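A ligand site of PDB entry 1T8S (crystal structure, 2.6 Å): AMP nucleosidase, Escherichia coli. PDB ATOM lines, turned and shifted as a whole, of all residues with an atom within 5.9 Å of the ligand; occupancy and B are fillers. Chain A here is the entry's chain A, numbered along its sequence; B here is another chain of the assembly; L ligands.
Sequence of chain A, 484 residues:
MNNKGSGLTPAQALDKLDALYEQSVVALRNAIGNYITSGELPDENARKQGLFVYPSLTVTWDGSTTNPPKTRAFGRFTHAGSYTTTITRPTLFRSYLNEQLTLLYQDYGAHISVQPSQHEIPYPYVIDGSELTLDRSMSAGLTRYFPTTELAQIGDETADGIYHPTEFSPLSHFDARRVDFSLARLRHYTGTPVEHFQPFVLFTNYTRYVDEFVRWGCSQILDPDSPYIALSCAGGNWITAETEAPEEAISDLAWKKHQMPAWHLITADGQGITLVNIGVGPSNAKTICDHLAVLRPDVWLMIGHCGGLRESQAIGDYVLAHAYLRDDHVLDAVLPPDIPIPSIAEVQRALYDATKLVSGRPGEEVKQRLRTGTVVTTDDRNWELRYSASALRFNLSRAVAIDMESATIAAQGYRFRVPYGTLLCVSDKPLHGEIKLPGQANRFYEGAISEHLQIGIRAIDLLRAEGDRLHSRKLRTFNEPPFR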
ATOM      1  N   ASN A 205      -4.846  11.354 -22.434  1.00  0.00           N
ATOM      2  CA  ASN A 205      -5.438  10.137 -22.942  1.00  0.00           C
ATOM      3  C   ASN A 205      -5.902  10.373 -24.357  1.00  0.00           C
ATOM      4  O   ASN A 205      -6.760   9.650 -24.862  1.00  0.00           O
ATOM      5  CB  ASN A 205      -6.621   9.730 -22.072  1.00  0.00           C
ATOM      6  CG  ASN A 205      -7.646  10.835 -21.911  1.00  0.00           C
ATOM      7  OD1 ASN A 205      -7.467  11.951 -22.415  1.00  0.00           O
ATOM      8  ND2 ASN A 205      -8.716  10.539 -21.188  1.00  0.00           N
ATOM      9  N   GLY A 279      -2.580   6.470 -22.615  1.00  0.00           N
ATOM     10  CA  GLY A 279      -3.470   5.496 -23.197  1.00  0.00           C
ATOM     11  C   GLY A 279      -4.765   5.426 -22.429  1.00  0.00           C
ATOM     12  O   GLY A 279      -5.208   6.439 -21.881  1.00  0.00           O
ATOM     13  N   VAL A 280      -5.375   4.249 -22.347  1.00  0.00           N
ATOM     14  CA  VAL A 280      -6.658   4.181 -21.652  1.00  0.00           C
ATOM     15  C   VAL A 280      -6.863   3.062 -20.619  1.00  0.00           C
ATOM     16  O   VAL A 280      -6.475   1.908 -20.816  1.00  0.00           O
ATOM     17  CB  VAL A 280      -7.818   4.128 -22.683  1.00  0.00           C
ATOM     18  CG1 VAL A 280      -7.393   3.348 -23.894  1.00  0.00           C
ATOM     19  CG2 VAL A 280      -9.043   3.482 -22.071  1.00  0.00           C
ATOM     20  N   GLY A 281      -7.507   3.445 -19.509  1.00  0.00           N
ATOM     21  CA  GLY A 281      -7.807   2.500 -18.451  1.00  0.00           C
ATOM     22  C   GLY A 281      -7.098   2.749 -17.139  1.00  0.00           C
ATOM     23  O   GLY A 281      -6.011   3.309 -17.114  1.00  0.00           O
ATOM     24  N   HIS A 305      -9.557  13.970 -21.989  1.00  0.00           N
ATOM     25  CA  HIS A 305     -10.972  13.986 -22.284  1.00  0.00           C
ATOM     26  C   HIS A 305     -11.811  13.305 -21.214  1.00  0.00           C
ATOM     27  O   HIS A 305     -11.296  12.510 -20.417  1.00  0.00           O
ATOM     28  CB  HIS A 305     -11.202  13.305 -23.640  1.00  0.00           C
ATOM     29  CG  HIS A 305     -10.727  14.138 -24.796  1.00  0.00           C
ATOM     30  ND1 HIS A 305     -10.783  13.697 -26.105  1.00  0.00           N
ATOM     31  CD2 HIS A 305     -10.228  15.400 -24.841  1.00  0.00           C
ATOM     32  CE1 HIS A 305     -10.351  14.657 -26.900  1.00  0.00           C
ATOM     33  NE2 HIS A 305     -10.006  15.695 -26.156  1.00  0.00           N
ATOM     34  N   CYS A 306     -13.105  13.613 -21.212  1.00  0.00           N
ATOM     35  CA  CYS A 306     -14.048  13.001 -20.277  1.00  0.00           C
ATOM     36  C   CYS A 306     -15.454  13.182 -20.826  1.00  0.00           C
ATOM     37  O   CYS A 306     -15.674  13.955 -21.748  1.00  0.00           O
ATOM     38  CB  CYS A 306     -13.968  13.666 -18.899  1.00  0.00           C
ATOM     39  SG  CYS A 306     -14.670  15.346 -18.833  1.00  0.00           S
ATOM     40  N   GLY A 307     -16.410  12.458 -20.254  1.00  0.00           N
ATOM     41  CA  GLY A 307     -17.783  12.590 -20.686  1.00  0.00           C
ATOM     42  C   GLY A 307     -18.473  13.532 -19.718  1.00  0.00           C
ATOM     43  O   GLY A 307     -18.304  13.380 -18.500  1.00  0.00           O
ATOM     44  N   THR A 378     -14.140   5.261 -13.951  1.00  0.00           N
ATOM     45  CA  THR A 378     -14.584   3.855 -14.007  1.00  0.00           C
ATOM     46  C   THR A 378     -13.640   2.971 -14.831  1.00  0.00           C
ATOM     47  O   THR A 378     -12.828   3.463 -15.615  1.00  0.00           O
ATOM     48  CB  THR A 378     -16.002   3.750 -14.626  1.00  0.00           C
ATOM     49  OG1 THR A 378     -16.413   2.373 -14.666  1.00  0.00           O
ATOM     50  CG2 THR A 378     -16.001   4.334 -16.037  1.00  0.00           C
ATOM     51  N   ASP A 380     -15.006   0.613 -16.566  1.00  0.00           N
ATOM     52  CA  ASP A 380     -16.002   0.105 -17.514  1.00  0.00           C
ATOM     53  C   ASP A 380     -16.403   1.168 -18.559  1.00  0.00           C
ATOM     54  O   ASP A 380     -17.380   1.908 -18.368  1.00  0.00           O
ATOM     55  CB  ASP A 380     -17.241  -0.355 -16.757  1.00  0.00           C
ATOM     56  CG  ASP A 380     -18.303  -0.925 -17.685  1.00  0.00           C
ATOM     57  OD1 ASP A 380     -17.985  -1.195 -18.857  1.00  0.00           O
ATOM     58  OD2 ASP A 380     -19.445  -1.122 -17.234  1.00  0.00           O
ATOM     59  N   ARG A 381     -15.645   1.246 -19.651  1.00  0.00           N
ATOM     60  CA  ARG A 381     -15.908   2.203 -20.717  1.00  0.00           C
ATOM     61  C   ARG A 381     -17.377   2.178 -21.136  1.00  0.00           C
ATOM     62  O   ARG A 381     -17.953   3.223 -21.387  1.00  0.00           O
ATOM     63  CB  ARG A 381     -15.032   1.912 -21.942  1.00  0.00           C
ATOM     64  CG  ARG A 381     -15.318   2.812 -23.146  1.00  0.00           C
ATOM     65  CD  ARG A 381     -14.887   4.245 -22.836  1.00  0.00           C
ATOM     66  NE  ARG A 381     -15.277   5.231 -23.862  1.00  0.00           N
ATOM     67  CZ  ARG A 381     -16.510   5.745 -23.999  1.00  0.00           C
ATOM     68  NH1 ARG A 381     -17.481   5.380 -23.180  1.00  0.00           N
ATOM     69  NH2 ARG A 381     -16.739   6.653 -24.939  1.00  0.00           N
ATOM     70  N   TRP A 383     -20.048   1.693 -19.429  1.00  0.00           N
ATOM     71  CA  TRP A 383     -20.965   1.845 -18.301  1.00  0.00           C
ATOM     72  C   TRP A 383     -22.365   2.241 -18.778  1.00  0.00           C
ATOM     73  O   TRP A 383     -23.353   1.926 -18.118  1.00  0.00           O
ATOM     74  CB  TRP A 383     -20.447   2.902 -17.329  1.00  0.00           C
ATOM     75  CG  TRP A 383     -20.220   4.227 -17.970  1.00  0.00           C
ATOM     76  CD1 TRP A 383     -19.074   4.668 -18.561  1.00  0.00           C
ATOM     77  CD2 TRP A 383     -21.183   5.267 -18.112  1.00  0.00           C
ATOM     78  NE1 TRP A 383     -19.259   5.939 -19.070  1.00  0.00           N
ATOM     79  CE2 TRP A 383     -20.550   6.328 -18.805  1.00  0.00           C
ATOM     80  CE3 TRP A 383     -22.518   5.416 -17.731  1.00  0.00           C
ATOM     81  CZ2 TRP A 383     -21.210   7.505 -19.123  1.00  0.00           C
ATOM     82  CZ3 TRP A 383     -23.176   6.592 -18.039  1.00  0.00           C
ATOM     83  CH2 TRP A 383     -22.520   7.632 -18.735  1.00  0.00           C
ATOM     84  N   GLU A 384     -22.474   2.923 -19.919  1.00  0.00           N
ATOM     85  CA  GLU A 384     -23.773   3.332 -20.441  1.00  0.00           C
ATOM     86  C   GLU A 384     -24.720   2.139 -20.592  1.00  0.00           C
ATOM     87  O   GLU A 384     -25.935   2.269 -20.411  1.00  0.00           O
ATOM     88  CB  GLU A 384     -23.631   4.024 -21.812  1.00  0.00           C
ATOM     89  CG  GLU A 384     -22.810   5.343 -21.803  1.00  0.00           C
ATOM     90  CD  GLU A 384     -21.313   5.150 -22.107  1.00  0.00           C
ATOM     91  OE1 GLU A 384     -20.737   4.121 -21.644  1.00  0.00           O
ATOM     92  OE2 GLU A 384     -20.719   6.040 -22.785  1.00  0.00           O
ATOM     93  N   ILE A 402     -17.250  11.853 -16.181  1.00  0.00           N
ATOM     94  CA  ILE A 402     -16.775  10.488 -16.039  1.00  0.00           C
ATOM     95  C   ILE A 402     -15.637  10.146 -17.009  1.00  0.00           C
ATOM     96  O   ILE A 402     -15.732  10.395 -18.217  1.00  0.00           O
ATOM     97  CB  ILE A 402     -17.912   9.516 -16.241  1.00  0.00           C
ATOM     98  CG1 ILE A 402     -17.414   8.083 -15.962  1.00  0.00           C
ATOM     99  CG2 ILE A 402     -18.469   9.632 -17.644  1.00  0.00           C
ATOM    100  CD1 ILE A 402     -18.543   7.009 -15.873  1.00  0.00           C
ATOM    101  N   ASP A 403     -14.546   9.598 -16.468  1.00  0.00           N
ATOM    102  CA  ASP A 403     -13.403   9.201 -17.297  1.00  0.00           C
ATOM    103  C   ASP A 403     -12.858   7.865 -16.802  1.00  0.00           C
ATOM    104  O   ASP A 403     -13.521   7.191 -16.011  1.00  0.00           O
ATOM    105  CB  ASP A 403     -12.310  10.276 -17.239  1.00  0.00           C
ATOM    106  CG  ASP A 403     -11.451  10.178 -15.993  1.00  0.00           C
ATOM    107  OD1 ASP A 403     -12.022   9.974 -14.898  1.00  0.00           O
ATOM    108  OD2 ASP A 403     -10.214  10.331 -16.115  1.00  0.00           O
ATOM    109  N   MET A 404     -11.675   7.491 -17.263  1.00  0.00           N
ATOM    110  CA  MET A 404     -11.087   6.213 -16.885  1.00  0.00           C
ATOM    111  C   MET A 404      -9.688   6.300 -16.303  1.00  0.00           C
ATOM    112  O   MET A 404      -9.047   5.263 -16.133  1.00  0.00           O
ATOM    113  CB  MET A 404     -11.096   5.262 -18.083  1.00  0.00           C
ATOM    114  CG  MET A 404     -12.495   4.928 -18.586  1.00  0.00           C
ATOM    115  SD  MET A 404     -12.535   3.802 -20.196  1.00  0.00           S
ATOM    116  CE  MET A 404     -12.050   2.071 -19.482  1.00  0.00           C
ATOM    117  N   GLU A 405      -9.200   7.489 -15.983  1.00  0.00           N
ATOM    118  CA  GLU A 405      -7.848   7.587 -15.445  1.00  0.00           C
ATOM    119  C   GLU A 405      -7.640   8.547 -14.276  1.00  0.00           C
ATOM    120  O   GLU A 405      -6.753   8.332 -13.449  1.00  0.00           O
ATOM    121  CB  GLU A 405      -6.861   7.989 -16.569  1.00  0.00           C
ATOM    122  CG  GLU A 405      -6.670   6.969 -17.697  1.00  0.00           C
ATOM    123  CD  GLU A 405      -7.704   7.106 -18.796  1.00  0.00           C
ATOM    124  OE1 GLU A 405      -8.153   8.255 -19.044  1.00  0.00           O
ATOM    125  OE2 GLU A 405      -8.073   6.079 -19.426  1.00  0.00           O
ATOM    126  N   SER A 427     -15.676  15.821 -23.948  1.00  0.00           N
ATOM    127  CA  SER A 427     -15.570  15.419 -25.341  1.00  0.00           C
ATOM    128  C   SER A 427     -16.848  14.772 -25.824  1.00  0.00           C
ATOM    129  O   SER A 427     -16.990  14.455 -26.998  1.00  0.00           O
ATOM    130  CB  SER A 427     -14.406  14.436 -25.501  1.00  0.00           C
ATOM    131  OG  SER A 427     -14.652  13.252 -24.766  1.00  0.00           O
ATOM    132  N   ASP A 428     -17.785  14.554 -24.908  1.00  0.00           N
ATOM    133  CA  ASP A 428     -19.056  13.946 -25.269  1.00  0.00           C
ATOM    134  C   ASP A 428     -20.061  14.072 -24.138  1.00  0.00           C
ATOM    135  O   ASP A 428     -19.704  14.385 -23.006  1.00  0.00           O
ATOM    136  CB  ASP A 428     -18.876  12.477 -25.651  1.00  0.00           C
ATOM    137  CG  ASP A 428     -18.300  11.640 -24.519  1.00  0.00           C
ATOM    138  OD1 ASP A 428     -17.116  11.824 -24.168  1.00  0.00           O
ATOM    139  OD2 ASP A 428     -19.042  10.773 -23.980  1.00  0.00           O
ATOM    140  N   PRO A 430     -22.801  11.564 -23.002  1.00  0.00           N
ATOM    141  CA  PRO A 430     -23.393  10.218 -22.974  1.00  0.00           C
ATOM    142  C   PRO A 430     -24.853  10.183 -22.576  1.00  0.00           C
ATOM    143  O   PRO A 430     -25.637   9.400 -23.122  1.00  0.00           O
ATOM    144  CB  PRO A 430     -22.531   9.480 -21.955  1.00  0.00           C
ATOM    145  CG  PRO A 430     -21.248  10.280 -21.887  1.00  0.00           C
ATOM    146  CD  PRO A 430     -21.737  11.680 -21.986  1.00  0.00           C
ATOM    147  N   LYS A 436     -20.673   9.055 -28.755  1.00  0.00           N
ATOM    148  CA  LYS A 436     -19.663   8.559 -29.687  1.00  0.00           C
ATOM    149  C   LYS A 436     -20.111   7.238 -30.328  1.00  0.00           C
ATOM    150  O   LYS A 436     -19.310   6.505 -30.907  1.00  0.00           O
ATOM    151  CB  LYS A 436     -18.329   8.346 -28.967  1.00  0.00           C
ATOM    152  CG  LYS A 436     -17.656   9.607 -28.441  1.00  0.00           C
ATOM    153  CD  LYS A 436     -16.314   9.279 -27.793  1.00  0.00           C
ATOM    154  CE  LYS A 436     -15.594  10.525 -27.325  1.00  0.00           C
ATOM    155  NZ  LYS A 436     -14.334  10.179 -26.595  1.00  0.00           N
ATOM    156  N   ARG B 185     -18.987   1.833 -32.991  1.00  0.00           N
ATOM    157  CA  ARG B 185     -17.836   1.744 -32.091  1.00  0.00           C
ATOM    158  C   ARG B 185     -16.722   0.822 -32.607  1.00  0.00           C
ATOM    159  O   ARG B 185     -15.526   1.121 -32.449  1.00  0.00           O
ATOM    160  CB  ARG B 185     -18.313   1.257 -30.720  1.00  0.00           C
ATOM    161  CG  ARG B 185     -17.992   2.214 -29.588  1.00  0.00           C
ATOM    162  CD  ARG B 185     -18.900   3.414 -29.525  1.00  0.00           C
ATOM    163  NE  ARG B 185     -18.708   4.081 -28.244  1.00  0.00           N
ATOM    164  CZ  ARG B 185     -19.617   4.831 -27.619  1.00  0.00           C
ATOM    165  NH1 ARG B 185     -20.804   5.031 -28.179  1.00  0.00           N
ATOM    166  NH2 ARG B 185     -19.352   5.363 -26.431  1.00  0.00           N
ATOM    167  N   HIS B 188     -14.589   2.605 -34.994  1.00  0.00           N
ATOM    168  CA  HIS B 188     -13.782   3.578 -34.267  1.00  0.00           C
ATOM    169  C   HIS B 188     -12.554   2.967 -33.584  1.00  0.00           C
ATOM    170  O   HIS B 188     -11.452   3.511 -33.683  1.00  0.00           O
ATOM    171  CB  HIS B 188     -14.659   4.275 -33.232  1.00  0.00           C
ATOM    172  CG  HIS B 188     -13.888   5.005 -32.178  1.00  0.00           C
ATOM    173  ND1 HIS B 188     -13.100   6.102 -32.459  1.00  0.00           N
ATOM    174  CD2 HIS B 188     -13.785   4.794 -30.841  1.00  0.00           C
ATOM    175  CE1 HIS B 188     -12.546   6.536 -31.335  1.00  0.00           C
ATOM    176  NE2 HIS B 188     -12.941   5.763 -30.352  1.00  0.00           N
ATOM    177  N   TYR B 189     -12.723   1.840 -32.890  1.00  0.00           N
ATOM    178  CA  TYR B 189     -11.585   1.225 -32.204  1.00  0.00           C
ATOM    179  C   TYR B 189     -10.670   0.448 -33.134  1.00  0.00           C
ATOM    180  O   TYR B 189      -9.453   0.389 -32.942  1.00  0.00           O
ATOM    181  CB  TYR B 189     -12.053   0.264 -31.101  1.00  0.00           C
ATOM    182  CG  TYR B 189     -12.786   0.916 -29.956  1.00  0.00           C
ATOM    183  CD1 TYR B 189     -12.176   1.916 -29.210  1.00  0.00           C
ATOM    184  CD2 TYR B 189     -14.079   0.544 -29.635  1.00  0.00           C
ATOM    185  CE1 TYR B 189     -12.845   2.532 -28.166  1.00  0.00           C
ATOM    186  CE2 TYR B 189     -14.766   1.150 -28.588  1.00  0.00           C
ATOM    187  CZ  TYR B 189     -14.146   2.146 -27.864  1.00  0.00           C
ATOM    188  OH  TYR B 189     -14.832   2.766 -26.848  1.00  0.00           O
ATOM    189  N   GLN B 259      -7.197   2.653 -31.086  1.00  0.00           N
ATOM    190  CA  GLN B 259      -6.841   1.992 -29.830  1.00  0.00           C
ATOM    191  C   GLN B 259      -6.645   0.490 -29.991  1.00  0.00           C
ATOM    192  O   GLN B 259      -5.757  -0.086 -29.359  1.00  0.00           O
ATOM    193  CB  GLN B 259      -7.919   2.269 -28.778  1.00  0.00           C
ATOM    194  CG  GLN B 259      -7.541   1.760 -27.412  1.00  0.00           C
ATOM    195  CD  GLN B 259      -8.677   1.837 -26.414  1.00  0.00           C
ATOM    196  OE1 GLN B 259      -8.641   1.171 -25.393  1.00  0.00           O
ATOM    197  NE2 GLN B 259      -9.690   2.658 -26.713  1.00  0.00           N
ATOM    198  N   THR B 287     -14.285  -3.910 -23.399  1.00  0.00           N
ATOM    199  CA  THR B 287     -14.837  -2.993 -24.382  1.00  0.00           C
ATOM    200  C   THR B 287     -14.926  -3.627 -25.779  1.00  0.00           C
ATOM    201  O   THR B 287     -16.001  -3.660 -26.388  1.00  0.00           O
ATOM    202  CB  THR B 287     -13.996  -1.698 -24.488  1.00  0.00           C
ATOM    203  OG1 THR B 287     -13.968  -1.030 -23.213  1.00  0.00           O
ATOM    204  CG2 THR B 287     -14.583  -0.738 -25.536  1.00  0.00           C
HETATM  205  P1  LIG L   1     -12.885   6.194 -26.364  1.00  0.00           P
HETATM  206  O1  LIG L   1     -13.288   4.790 -26.052  1.00  0.00           O
HETATM  207  O2  LIG L   1     -12.245   6.378 -27.701  1.00  0.00           O
HETATM  208  O3  LIG L   1     -13.917   7.234 -26.031  1.00  0.00           O
HETATM  209  O4  LIG L   1     -11.751   6.519 -25.337  1.00  0.00           O
HETATM  210  C1  LIG L   1     -11.788   6.476 -23.916  1.00  0.00           C
HETATM  211  C2  LIG L   1     -11.046   7.635 -23.240  1.00  0.00           C
HETATM  212  O5  LIG L   1     -11.996   8.708 -23.161  1.00  0.00           O
HETATM  213  C3  LIG L   1     -10.586   7.223 -21.815  1.00  0.00           C
HETATM  214  O6  LIG L   1      -9.191   7.525 -21.625  1.00  0.00           O
HETATM  215  C4  LIG L   1     -11.417   8.043 -20.856  1.00  0.00           C
HETATM  216  O7  LIG L   1     -10.651   8.707 -19.853  1.00  0.00           O
HETATM  217  C5  LIG L   1     -12.227   8.940 -21.781  1.00  0.00           C
HETATM  218  C6  LIG L   1     -13.703   9.076 -21.864  1.00  0.00           C
HETATM  219  N1  LIG L   1     -14.294  10.005 -22.588  1.00  0.00           N
HETATM  220  N2  LIG L   1     -15.622   9.949 -22.553  1.00  0.00           N
HETATM  221  C7  LIG L   1     -17.135   8.297 -21.289  1.00  0.00           C
HETATM  222  N3  LIG L   1     -18.309   8.777 -21.708  1.00  0.00           N
HETATM  223  C8  LIG L   1     -15.914   8.891 -21.729  1.00  0.00           C
HETATM  224  C9  LIG L   1     -14.746   8.325 -21.280  1.00  0.00           C
HETATM  225  N4  LIG L   1     -14.652   7.225 -20.422  1.00  0.00           N
HETATM  226  C10 LIG L   1     -15.865   6.758 -20.074  1.00  0.00           C
HETATM  227  N5  LIG L   1     -17.071   7.204 -20.447  1.00  0.00           N
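The side-chain amide nitrogen of Asn 205 is in hydrogen-bond range of an oxygen (O7) of the ligand (3.0 Å). The side-chain hydroxyl of Tyr 189 of chain B is in hydrogen-bond range of an oxygen (O1) of the ligand (2.7 Å). N2 of the ligand is in hydrogen-bond range of OD1 of Asp 428. O2 of the ligand sits at hydrogen-bond distance from NE2 of His 188 of chain B (2.8 Å). O7 of the ligand sits at hydrogen-bond distance from OE1 of Glu 405. NE of Arg 381 is in salt-bridge range of O1 of the ligand (3.0 Å). NZ of Lys 436 lies within salt-bridge range of O3 of the ligand (3.0 Å). N of Gly 307 lies close to N2 of the ligand, at 3.5 Å. The indole nitrogen (NE1) of Trp 383 lies within hydrogen-bond range of a nitrogen (N5) of the ligand, 2.9 Å away. The backbone NH of Met 404 sits at hydrogen-bond distance from an oxygen (O7) of the ligand (3.0 Å).
The side-chain carboxylate of Glu 384 is in hydrogen-bond range of the indole nitrogen of Trp 383, 3.5 Å away. The backbone NH (N) of Ser 427 sits at hydrogen-bond distance from the backbone carbonyl oxygen (O) of Cys 306, 2.9 Å away. The guanidinium group of Arg 381 is in salt-bridge range of the side-chain carboxylate of Glu 384 (3.3 Å). NH1 of Arg 185 of chain B lies close to O of Lys 436, 3.4 Å away. OD2 of Asp 403 lies within hydrogen-bond range of N of Glu 405, at 3.0 Å. The backbone carbonyl oxygen (O) of Asp 403 is in hydrogen-bond range of the backbone NH (N) of Thr 378, 2.9 Å away. The side-chain hydroxyl (OG) of Ser 427 lies within hydrogen-bond range of the side-chain carboxylate (OD1) of Asp 428, at 2.9 Å. OE2 of Glu 405 lies within hydrogen-bond range of N of Gly 281, 2.7 Å away.
Residues that only touch the ligand: Val 280 (3.8 Å), His 305 (3.9 Å), Cys 306 (3.7 Å), Glu 384 (3.8 Å), Ile 402 (3.8 Å), Asp 403 (3.5 Å), Ser 427 (3.9 Å) and Pro 430 (3.3 Å). 18 residues have an atom within 4 Å of the ligand: Asn 205, Val 280, His 305, Cys 306, Gly 307, Arg 381, Trp 383, Glu 384, Ile 402, Asp 403, Met 404, Glu 405, Ser 427, Asp 428, Pro 430, Lys 436, His 188 of chain B and Tyr 189 of chain B.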
